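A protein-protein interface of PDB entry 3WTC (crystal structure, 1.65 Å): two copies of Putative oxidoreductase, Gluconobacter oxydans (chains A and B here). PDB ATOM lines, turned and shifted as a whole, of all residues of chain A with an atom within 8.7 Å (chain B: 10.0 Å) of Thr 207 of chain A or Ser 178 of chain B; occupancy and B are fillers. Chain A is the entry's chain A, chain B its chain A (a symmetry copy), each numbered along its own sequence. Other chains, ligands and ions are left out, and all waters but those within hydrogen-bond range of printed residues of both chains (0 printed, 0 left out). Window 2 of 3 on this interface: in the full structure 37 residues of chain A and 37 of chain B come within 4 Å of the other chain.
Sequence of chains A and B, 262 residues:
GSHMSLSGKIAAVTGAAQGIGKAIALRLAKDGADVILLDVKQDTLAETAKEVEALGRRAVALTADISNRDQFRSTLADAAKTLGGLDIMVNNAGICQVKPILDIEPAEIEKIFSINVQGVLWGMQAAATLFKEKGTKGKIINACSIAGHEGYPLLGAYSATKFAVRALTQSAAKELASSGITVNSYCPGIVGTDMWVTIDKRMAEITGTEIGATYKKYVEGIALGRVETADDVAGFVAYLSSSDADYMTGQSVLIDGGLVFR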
ATOM      1  N   PRO A 100      16.163  -0.816  -5.388  1.00  0.00           N
ATOM      2  CA  PRO A 100      14.763  -0.767  -5.795  1.00  0.00           C
ATOM      3  C   PRO A 100      14.551  -1.365  -7.165  1.00  0.00           C
ATOM      4  O   PRO A 100      15.447  -1.269  -8.006  1.00  0.00           O
ATOM      5  CB  PRO A 100      14.451   0.714  -5.843  1.00  0.00           C
ATOM      6  CG  PRO A 100      15.435   1.353  -5.072  1.00  0.00           C
ATOM      7  CD  PRO A 100      16.675   0.513  -5.075  1.00  0.00           C
ATOM      8  N   PRO A 153      10.477  -5.823  -0.455  1.00  0.00           N
ATOM      9  CA  PRO A 153      10.873  -4.546  -1.044  1.00  0.00           C
ATOM     10  C   PRO A 153      12.378  -4.303  -0.904  1.00  0.00           C
ATOM     11  O   PRO A 153      13.029  -4.700   0.075  1.00  0.00           O
ATOM     12  CB  PRO A 153      10.047  -3.562  -0.272  1.00  0.00           C
ATOM     13  CG  PRO A 153       9.834  -4.189   1.038  1.00  0.00           C
ATOM     14  CD  PRO A 153       9.690  -5.664   0.761  1.00  0.00           C
ATOM     15  N   LEU A 154      12.941  -3.780  -1.982  1.00  0.00           N
ATOM     16  CA  LEU A 154      14.346  -3.506  -2.169  1.00  0.00           C
ATOM     17  C   LEU A 154      15.208  -4.739  -2.341  1.00  0.00           C
ATOM     18  O   LEU A 154      16.422  -4.659  -2.491  1.00  0.00           O
ATOM     19  CB  LEU A 154      14.924  -2.587  -1.075  1.00  0.00           C
ATOM     20  CG  LEU A 154      14.688  -1.077  -1.146  1.00  0.00           C
ATOM     21  CD1 LEU A 154      13.434  -0.602  -1.751  1.00  0.00           C
ATOM     22  CD2 LEU A 154      14.854  -0.480   0.220  1.00  0.00           C
ATOM     23  N   ILE A 199      17.763  -1.018   4.140  1.00  0.00           N
ATOM     24  CA  ILE A 199      16.554  -1.203   3.388  1.00  0.00           C
ATOM     25  C   ILE A 199      15.516  -0.242   3.930  1.00  0.00           C
ATOM     26  O   ILE A 199      14.792   0.440   3.184  1.00  0.00           O
ATOM     27  CB  ILE A 199      16.019  -2.657   3.499  1.00  0.00           C
ATOM     28  CG1 ILE A 199      16.794  -3.621   2.565  1.00  0.00           C
ATOM     29  CG2 ILE A 199      14.534  -2.672   3.213  1.00  0.00           C
ATOM     30  CD1 ILE A 199      16.609  -5.072   2.938  1.00  0.00           C
ATOM     31  N   ASP A 200      15.387  -0.150   5.259  1.00  0.00           N
ATOM     32  CA  ASP A 200      14.370   0.730   5.866  1.00  0.00           C
ATOM     33  C   ASP A 200      14.485   2.221   5.437  1.00  0.00           C
ATOM     34  O   ASP A 200      13.444   2.867   5.112  1.00  0.00           O
ATOM     35  CB  ASP A 200      14.421   0.631   7.413  1.00  0.00           C
ATOM     36  CG  ASP A 200      13.445   1.591   8.104  1.00  0.00           C
ATOM     37  OD1 ASP A 200      13.776   2.844   8.098  1.00  0.00           O
ATOM     38  OD2 ASP A 200      12.389   1.102   8.634  1.00  0.00           O
ATOM     39  N   LYS A 201      15.736   2.716   5.423  1.00  0.00           N
ATOM     40  CA  LYS A 201      16.010   4.080   5.016  1.00  0.00           C
ATOM     41  C   LYS A 201      15.584   4.220   3.546  1.00  0.00           C
ATOM     42  O   LYS A 201      14.759   5.080   3.196  1.00  0.00           O
ATOM     43  CB  LYS A 201      17.502   4.395   5.149  1.00  0.00           C
ATOM     44  CG  LYS A 201      17.800   5.779   4.557  1.00  0.00           C
ATOM     45  CD  LYS A 201      19.149   6.345   4.942  1.00  0.00           C
ATOM     46  CE  LYS A 201      19.172   7.861   4.724  1.00  0.00           C
ATOM     47  NZ  LYS A 201      20.325   8.453   5.434  1.00  0.00           N
ATOM     48  N   ARG A 202      16.144   3.339   2.707  1.00  0.00           N
ATOM     49  CA  ARG A 202      15.912   3.454   1.283  1.00  0.00           C
ATOM     50  C   ARG A 202      14.433   3.288   0.942  1.00  0.00           C
ATOM     51  O   ARG A 202      13.947   3.960   0.019  1.00  0.00           O
ATOM     52  CB  ARG A 202      16.833   2.544   0.468  1.00  0.00           C
ATOM     53  CG  ARG A 202      18.184   3.188   0.220  1.00  0.00           C
ATOM     54  CD  ARG A 202      19.015   2.354  -0.740  1.00  0.00           C
ATOM     55  NE  ARG A 202      20.343   2.054  -0.205  1.00  0.00           N
ATOM     56  CZ  ARG A 202      21.223   1.255  -0.798  1.00  0.00           C
ATOM     57  NH1 ARG A 202      20.936   0.675  -1.972  1.00  0.00           N
ATOM     58  NH2 ARG A 202      22.399   1.043  -0.218  1.00  0.00           N
ATOM     59  N   MET A 203      13.686   2.482   1.700  1.00  0.00           N
ATOM     60  CA  MET A 203      12.220   2.359   1.448  1.00  0.00           C
ATOM     61  C   MET A 203      11.479   3.693   1.655  1.00  0.00           C
ATOM     62  O   MET A 203      10.574   4.045   0.886  1.00  0.00           O
ATOM     63  CB  MET A 203      11.550   1.298   2.366  1.00  0.00           C
ATOM     64  CG  MET A 203      11.306  -0.047   1.747  1.00  0.00           C
ATOM     65  SD  MET A 203      10.206   0.034   0.282  1.00  0.00           S
ATOM     66  CE  MET A 203       8.550  -0.189   0.926  1.00  0.00           C
ATOM     67  N   ALA A 204      11.851   4.415   2.719  1.00  0.00           N
ATOM     68  CA  ALA A 204      11.287   5.732   3.021  1.00  0.00           C
ATOM     69  C   ALA A 204      11.555   6.711   1.868  1.00  0.00           C
ATOM     70  O   ALA A 204      10.640   7.404   1.385  1.00  0.00           O
ATOM     71  CB  ALA A 204      11.887   6.250   4.336  1.00  0.00           C
ATOM     72  N   GLU A 205      12.815   6.764   1.435  1.00  0.00           N
ATOM     73  CA  GLU A 205      13.222   7.611   0.305  1.00  0.00           C
ATOM     74  C   GLU A 205      12.393   7.229  -0.952  1.00  0.00           C
ATOM     75  O   GLU A 205      11.800   8.092  -1.576  1.00  0.00           O
ATOM     76  CB  GLU A 205      14.738   7.512   0.051  1.00  0.00           C
ATOM     77  CG  GLU A 205      15.623   8.134   1.133  1.00  0.00           C
ATOM     78  CD  GLU A 205      17.086   7.607   1.170  1.00  0.00           C
ATOM     79  OE1 GLU A 205      17.462   6.628   0.467  1.00  0.00           O
ATOM     80  OE2 GLU A 205      17.889   8.165   1.950  1.00  0.00           O
ATOM     81  N   ILE A 206      12.288   5.948  -1.307  1.00  0.00           N
ATOM     82  CA  ILE A 206      11.634   5.601  -2.611  1.00  0.00           C
ATOM     83  C   ILE A 206      10.105   5.448  -2.650  1.00  0.00           C
ATOM     84  O   ILE A 206       9.532   5.564  -3.735  1.00  0.00           O
ATOM     85  CB  ILE A 206      12.258   4.347  -3.308  1.00  0.00           C
ATOM     86  CG1 ILE A 206      11.830   3.023  -2.618  1.00  0.00           C
ATOM     87  CG2 ILE A 206      13.770   4.538  -3.451  1.00  0.00           C
ATOM     88  CD1 ILE A 206      11.148   2.021  -3.546  1.00  0.00           C
ATOM     89  N   THR A 207       9.466   5.141  -1.506  1.00  0.00           N
ATOM     90  CA  THR A 207       7.996   4.968  -1.399  1.00  0.00           C
ATOM     91  C   THR A 207       7.315   5.971  -0.449  1.00  0.00           C
ATOM     92  O   THR A 207       6.101   5.940  -0.336  1.00  0.00           O
ATOM     93  CB  THR A 207       7.579   3.575  -0.824  1.00  0.00           C
ATOM     94  OG1 THR A 207       8.157   3.400   0.485  1.00  0.00           O
ATOM     95  CG2 THR A 207       7.977   2.415  -1.746  1.00  0.00           C
ATOM     96  N   GLY A 208       8.083   6.807   0.264  1.00  0.00           N
ATOM     97  CA  GLY A 208       7.511   7.718   1.282  1.00  0.00           C
ATOM     98  C   GLY A 208       7.027   7.037   2.571  1.00  0.00           C
ATOM     99  O   GLY A 208       6.209   7.598   3.298  1.00  0.00           O
ATOM    100  N   THR A 209       7.509   5.823   2.853  1.00  0.00           N
ATOM    101  CA  THR A 209       7.298   5.186   4.171  1.00  0.00           C
ATOM    102  C   THR A 209       8.015   6.042   5.240  1.00  0.00           C
ATOM    103  O   THR A 209       8.964   6.766   4.915  1.00  0.00           O
ATOM    104  CB  THR A 209       7.892   3.740   4.214  1.00  0.00           C
ATOM    105  OG1 THR A 209       7.369   2.963   3.130  1.00  0.00           O
ATOM    106  CG2 THR A 209       7.561   3.030   5.518  1.00  0.00           C
ATOM    107  N   GLU A 210       7.562   5.959   6.492  1.00  0.00           N
ATOM    108  CA  GLU A 210       8.280   6.573   7.628  1.00  0.00           C
ATOM    109  C   GLU A 210       9.590   5.835   7.953  1.00  0.00           C
ATOM    110  O   GLU A 210       9.657   4.592   7.848  1.00  0.00           O
ATOM    111  CB  GLU A 210       7.375   6.605   8.869  1.00  0.00           C
ATOM    112  CG  GLU A 210       6.113   7.452   8.676  1.00  0.00           C
ATOM    113  CD  GLU A 210       5.791   8.362   9.866  1.00  0.00           C
ATOM    114  OE1 GLU A 210       6.656   8.552  10.756  1.00  0.00           O
ATOM    115  OE2 GLU A 210       4.665   8.909   9.913  1.00  0.00           O
ATOM    116  N   THR A 214       9.820   0.128   8.308  1.00  0.00           N
ATOM    117  CA  THR A 214      10.117  -1.120   7.577  1.00  0.00           C
ATOM    118  C   THR A 214      10.907  -2.099   8.489  1.00  0.00           C
ATOM    119  O   THR A 214      10.674  -3.342   8.484  1.00  0.00           O
ATOM    120  CB  THR A 214      10.838  -0.810   6.235  1.00  0.00           C
ATOM    121  OG1 THR A 214       9.990   0.070   5.470  1.00  0.00           O
ATOM    122  CG2 THR A 214      11.165  -2.146   5.400  1.00  0.00           C
ATOM    123  N   LYS B 132       5.029   6.962 -13.712  1.00  0.00           N
ATOM    124  CA  LYS B 132       5.449   7.837 -12.632  1.00  0.00           C
ATOM    125  C   LYS B 132       5.736   9.209 -13.184  1.00  0.00           C
ATOM    126  O   LYS B 132       5.337  10.165 -12.572  1.00  0.00           O
ATOM    127  CB  LYS B 132       6.672   7.362 -11.923  1.00  0.00           C
ATOM    128  CG  LYS B 132       6.347   6.198 -10.952  1.00  0.00           C
ATOM    129  CD  LYS B 132       7.538   5.511 -10.364  1.00  0.00           C
ATOM    130  CE  LYS B 132       8.296   6.416  -9.417  1.00  0.00           C
ATOM    131  NZ  LYS B 132       7.410   6.908  -8.311  1.00  0.00           N
ATOM    132  N   GLY B 135       2.485  10.612 -13.684  1.00  0.00           N
ATOM    133  CA  GLY B 135       1.478  10.474 -12.607  1.00  0.00           C
ATOM    134  C   GLY B 135       0.307   9.509 -12.845  1.00  0.00           C
ATOM    135  O   GLY B 135      -0.657   9.464 -12.117  1.00  0.00           O
ATOM    136  N   THR B 136       0.399   8.621 -13.792  1.00  0.00           N
ATOM    137  CA  THR B 136      -0.770   7.774 -14.071  1.00  0.00           C
ATOM    138  C   THR B 136      -0.799   6.586 -13.090  1.00  0.00           C
ATOM    139  O   THR B 136       0.252   6.108 -12.689  1.00  0.00           O
ATOM    140  CB  THR B 136      -0.833   7.392 -15.575  1.00  0.00           C
ATOM    141  OG1 THR B 136      -1.106   5.987 -15.845  1.00  0.00           O
ATOM    142  CG2 THR B 136       0.327   7.886 -16.347  1.00  0.00           C
ATOM    143  N   LYS B 137      -2.009   6.137 -12.730  1.00  0.00           N
ATOM    144  CA  LYS B 137      -2.250   4.909 -11.946  1.00  0.00           C
ATOM    145  C   LYS B 137      -2.198   3.627 -12.758  1.00  0.00           C
ATOM    146  O   LYS B 137      -3.193   3.065 -13.132  1.00  0.00           O
ATOM    147  CB  LYS B 137      -3.625   4.928 -11.341  1.00  0.00           C
ATOM    148  CG  LYS B 137      -3.658   5.997 -10.261  1.00  0.00           C
ATOM    149  CD  LYS B 137      -5.066   6.180  -9.728  1.00  0.00           C
ATOM    150  CE  LYS B 137      -5.095   7.313  -8.673  1.00  0.00           C
ATOM    151  NZ  LYS B 137      -6.300   7.182  -7.807  1.00  0.00           N
ATOM    152  N   GLY B 138      -1.039   3.194 -13.052  1.00  0.00           N
ATOM    153  CA  GLY B 138      -0.969   2.204 -14.099  1.00  0.00           C
ATOM    154  C   GLY B 138      -1.077   0.781 -13.576  1.00  0.00           C
ATOM    155  O   GLY B 138      -1.046   0.480 -12.358  1.00  0.00           O
ATOM    156  N   SER B 171       7.698  -8.139  -5.255  1.00  0.00           N
ATOM    157  CA  SER B 171       8.588  -7.004  -4.796  1.00  0.00           C
ATOM    158  C   SER B 171       8.114  -5.712  -5.438  1.00  0.00           C
ATOM    159  O   SER B 171       8.019  -4.649  -4.785  1.00  0.00           O
ATOM    160  CB  SER B 171      10.054  -7.274  -5.126  1.00  0.00           C
ATOM    161  OG  SER B 171      10.545  -8.338  -4.349  1.00  0.00           O
ATOM    162  N   ALA B 172       7.822  -5.755  -6.715  1.00  0.00           N
ATOM    163  CA  ALA B 172       7.337  -4.584  -7.452  1.00  0.00           C
ATOM    164  C   ALA B 172       6.005  -4.120  -6.962  1.00  0.00           C
ATOM    165  O   ALA B 172       5.776  -2.896  -6.786  1.00  0.00           O
ATOM    166  CB  ALA B 172       7.357  -4.801  -8.935  1.00  0.00           C
ATOM    167  N   ALA B 173       5.101  -5.025  -6.630  1.00  0.00           N
ATOM    168  CA  ALA B 173       3.824  -4.621  -6.119  1.00  0.00           C
ATOM    169  C   ALA B 173       4.038  -3.820  -4.815  1.00  0.00           C
ATOM    170  O   ALA B 173       3.413  -2.784  -4.610  1.00  0.00           O
ATOM    171  CB  ALA B 173       2.899  -5.797  -5.888  1.00  0.00           C
ATOM    172  N   LYS B 174       4.917  -4.297  -3.960  1.00  0.00           N
ATOM    173  CA  LYS B 174       5.163  -3.643  -2.669  1.00  0.00           C
ATOM    174  C   LYS B 174       5.807  -2.288  -2.853  1.00  0.00           C
ATOM    175  O   LYS B 174       5.450  -1.330  -2.102  1.00  0.00           O
ATOM    176  CB  LYS B 174       6.009  -4.532  -1.781  1.00  0.00           C
ATOM    177  CG  LYS B 174       5.253  -5.771  -1.333  1.00  0.00           C
ATOM    178  CD  LYS B 174       6.104  -6.637  -0.457  1.00  0.00           C
ATOM    179  CE  LYS B 174       5.327  -7.890  -0.019  1.00  0.00           C
ATOM    180  NZ  LYS B 174       6.243  -8.647   0.872  1.00  0.00           N
ATOM    181  N   GLU B 175       6.687  -2.149  -3.842  1.00  0.00           N
ATOM    182  CA  GLU B 175       7.448  -0.903  -4.007  1.00  0.00           C
ATOM    183  C   GLU B 175       6.675   0.137  -4.769  1.00  0.00           C
ATOM    184  O   GLU B 175       6.930   1.372  -4.560  1.00  0.00           O
ATOM    185  CB  GLU B 175       8.758  -1.158  -4.702  1.00  0.00           C
ATOM    186  CG  GLU B 175       9.762  -1.950  -3.893  1.00  0.00           C
ATOM    187  CD  GLU B 175      11.042  -2.270  -4.687  1.00  0.00           C
ATOM    188  OE1 GLU B 175      11.465  -1.464  -5.569  1.00  0.00           O
ATOM    189  OE2 GLU B 175      11.650  -3.305  -4.340  1.00  0.00           O
ATOM    190  N   LEU B 176       5.770  -0.244  -5.682  1.00  0.00           N
ATOM    191  CA  LEU B 176       5.099   0.664  -6.580  1.00  0.00           C
ATOM    192  C   LEU B 176       3.719   1.045  -6.111  1.00  0.00           C
ATOM    193  O   LEU B 176       3.128   1.948  -6.732  1.00  0.00           O
ATOM    194  CB  LEU B 176       5.102   0.100  -7.989  1.00  0.00           C
ATOM    195  CG  LEU B 176       6.465  -0.136  -8.643  1.00  0.00           C
ATOM    196  CD1 LEU B 176       6.264  -0.762 -10.012  1.00  0.00           C
ATOM    197  CD2 LEU B 176       7.252   1.163  -8.702  1.00  0.00           C
ATOM    198  N   ALA B 177       3.183   0.370  -5.078  1.00  0.00           N
ATOM    199  CA  ALA B 177       1.826   0.660  -4.608  1.00  0.00           C
ATOM    200  C   ALA B 177       1.690   2.142  -4.247  1.00  0.00           C
ATOM    201  O   ALA B 177       0.638   2.722  -4.555  1.00  0.00           O
ATOM    202  CB  ALA B 177       1.429  -0.201  -3.460  1.00  0.00           C
ATOM    203  N   SER B 178       2.731   2.726  -3.655  1.00  0.00           N
ATOM    204  CA  SER B 178       2.589   4.124  -3.194  1.00  0.00           C
ATOM    205  C   SER B 178       2.623   5.093  -4.341  1.00  0.00           C
ATOM    206  O   SER B 178       2.305   6.297  -4.098  1.00  0.00           O
ATOM    207  CB  SER B 178       3.639   4.480  -2.125  1.00  0.00           C
ATOM    208  OG  SER B 178       4.907   4.410  -2.698  1.00  0.00           O
ATOM    209  N   SER B 179       2.942   4.690  -5.558  1.00  0.00           N
ATOM    210  CA  SER B 179       2.803   5.450  -6.743  1.00  0.00           C
ATOM    211  C   SER B 179       1.512   5.171  -7.486  1.00  0.00           C
ATOM    212  O   SER B 179       1.347   5.581  -8.621  1.00  0.00           O
ATOM    213  CB  SER B 179       3.950   5.157  -7.694  1.00  0.00           C
ATOM    214  OG  SER B 179       5.187   5.439  -7.056  1.00  0.00           O
ATOM    215  N   GLY B 180       0.619   4.397  -6.907  1.00  0.00           N
ATOM    216  CA  GLY B 180      -0.611   4.053  -7.553  1.00  0.00           C
ATOM    217  C   GLY B 180      -0.586   3.020  -8.666  1.00  0.00           C
ATOM    218  O   GLY B 180      -1.446   3.006  -9.526  1.00  0.00           O
ATOM    219  N   ILE B 181       0.427   2.179  -8.615  1.00  0.00           N
ATOM    220  CA  ILE B 181       0.649   1.192  -9.673  1.00  0.00           C
ATOM    221  C   ILE B 181       0.453  -0.171  -9.036  1.00  0.00           C
ATOM    222  O   ILE B 181       1.086  -0.474  -8.010  1.00  0.00           O
ATOM    223  CB  ILE B 181       2.062   1.335 -10.225  1.00  0.00           C
ATOM    224  CG1 ILE B 181       2.222   2.676 -10.930  1.00  0.00           C
ATOM    225  CG2 ILE B 181       2.348   0.206 -11.227  1.00  0.00           C
ATOM    226  CD1 ILE B 181       3.687   3.116 -11.046  1.00  0.00           C
ATOM    227  N   THR B 182      -0.323  -1.011  -9.713  1.00  0.00           N
ATOM    228  CA  THR B 182      -0.506  -2.401  -9.317  1.00  0.00           C
ATOM    229  C   THR B 182       0.332  -3.312 -10.205  1.00  0.00           C
ATOM    230  O   THR B 182       0.608  -2.994 -11.360  1.00  0.00           O
ATOM    231  CB  THR B 182      -1.949  -2.850  -9.364  1.00  0.00           C
ATOM    232  OG1 THR B 182      -2.478  -2.784 -10.711  1.00  0.00           O
ATOM    233  CG2 THR B 182      -2.853  -2.034  -8.479  1.00  0.00           C
ATOM    234  N   VAL B 183       0.703  -4.439  -9.629  1.00  0.00           N
ATOM    235  CA  VAL B 183       1.524  -5.437 -10.348  1.00  0.00           C
ATOM    236  C   VAL B 183       0.956  -6.787 -10.002  1.00  0.00           C
ATOM    237  O   VAL B 183       0.975  -7.183  -8.834  1.00  0.00           O
ATOM    238  CB  VAL B 183       2.997  -5.352  -9.922  1.00  0.00           C
ATOM    239  CG1 VAL B 183       3.848  -6.143 -10.859  1.00  0.00           C
ATOM    240  CG2 VAL B 183       3.551  -3.908  -9.946  1.00  0.00           C
ATOM    241  N   THR B 249      -3.403  -6.539  -6.023  1.00  0.00           N
ATOM    242  CA  THR B 249      -1.978  -6.363  -6.305  1.00  0.00           C
ATOM    243  C   THR B 249      -1.102  -7.393  -5.619  1.00  0.00           C
ATOM    244  O   THR B 249      -1.462  -7.940  -4.577  1.00  0.00           O
ATOM    245  CB  THR B 249      -1.481  -4.919  -5.957  1.00  0.00           C
ATOM    246  OG1 THR B 249      -0.263  -4.646  -6.727  1.00  0.00           O
ATOM    247  CG2 THR B 249      -1.237  -4.726  -4.459  1.00  0.00           C
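The side-chain carboxylate (OE2) of Glu 175 of chain B sits at hydrogen-bond distance from the backbone NH (N) of Leu 154 of chain A, at 2.7 Å. The backbone carbonyl oxygen (O) of Thr 207 of chain A lies within hydrogen-bond range of the side-chain hydroxyl (OG) of Ser 178 of chain B (3.1 Å).
OG1 of Thr 207 of chain A lies within hydrogen-bond range of O of Met 203 of chain A, at 2.5 Å. The side-chain hydroxyl of Thr 209 of chain A lies within hydrogen-bond range of the side-chain hydroxyl of Thr 207 of chain A, at 2.8 Å.
Pro 100 of chain A touches Glu 175 of chain B (CA to OE1, 3.4 Å). Pro 153 of chain A touches Lys 174 of chain B. Glu 175 of chain B touches Pro 153 of chain A. CG2 of Thr 207 of chain A touches O of Glu 175 of chain B, at 3.2 Å.
Of chain B, only Glu 175 and Ser 178 come within 4 Å of Thr 207 of chain A. Ser 178 of chain B touches just one residue of chain A: Thr 207 (3.1 Å). Of the printed residues of chain A, Lys 174 of chain B touches Pro 153 (3.9 Å). Printed residues of chain A within 4 Å of Glu 175 of chain B: Pro 100 (3.4 Å), Pro 153 (3.6 Å), Leu 154 (2.7 Å) and Thr 207 (3.2 Å). Of the printed residues of chain B, Pro 100 of chain A touches Glu 175 (3.4 Å). Printed residues of chain B within 4 Å of Pro 153 of chain A: Lys 174 (3.9 Å) and Glu 175 (3.6 Å). Of the printed residues of chain B, Leu 154 of chain A touches Glu 175. Ile 181 of chain B touches none of the printed residues of chain A. Val 183 of chain B touches none of the printed residues of chain A. The nearest printed residue of chain A that does not touch Lys 174 of chain B is Met 203 of chain A (4.5 Å).
Of the 19 printed residues of chain B, 3 touch a printed residue of chain A. Printed residues of chain B that touch a printed residue of chain A: Lys 174, Glu 175 and Ser 178. Of the 16 printed residues of chain A, 4 touch a printed residue of chain B. Printed residues of chain A that touch a printed residue of chain B: Pro 100, Pro 153, Leu 154 and Thr 207. Among the printed residues, 6 pairs touch across the chains. Among the printed residues, no Asp or Glu carboxylate lies within 4 Å of a Lys or Arg side-chain nitrogen of the other chain.
No position is printed for both chains.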
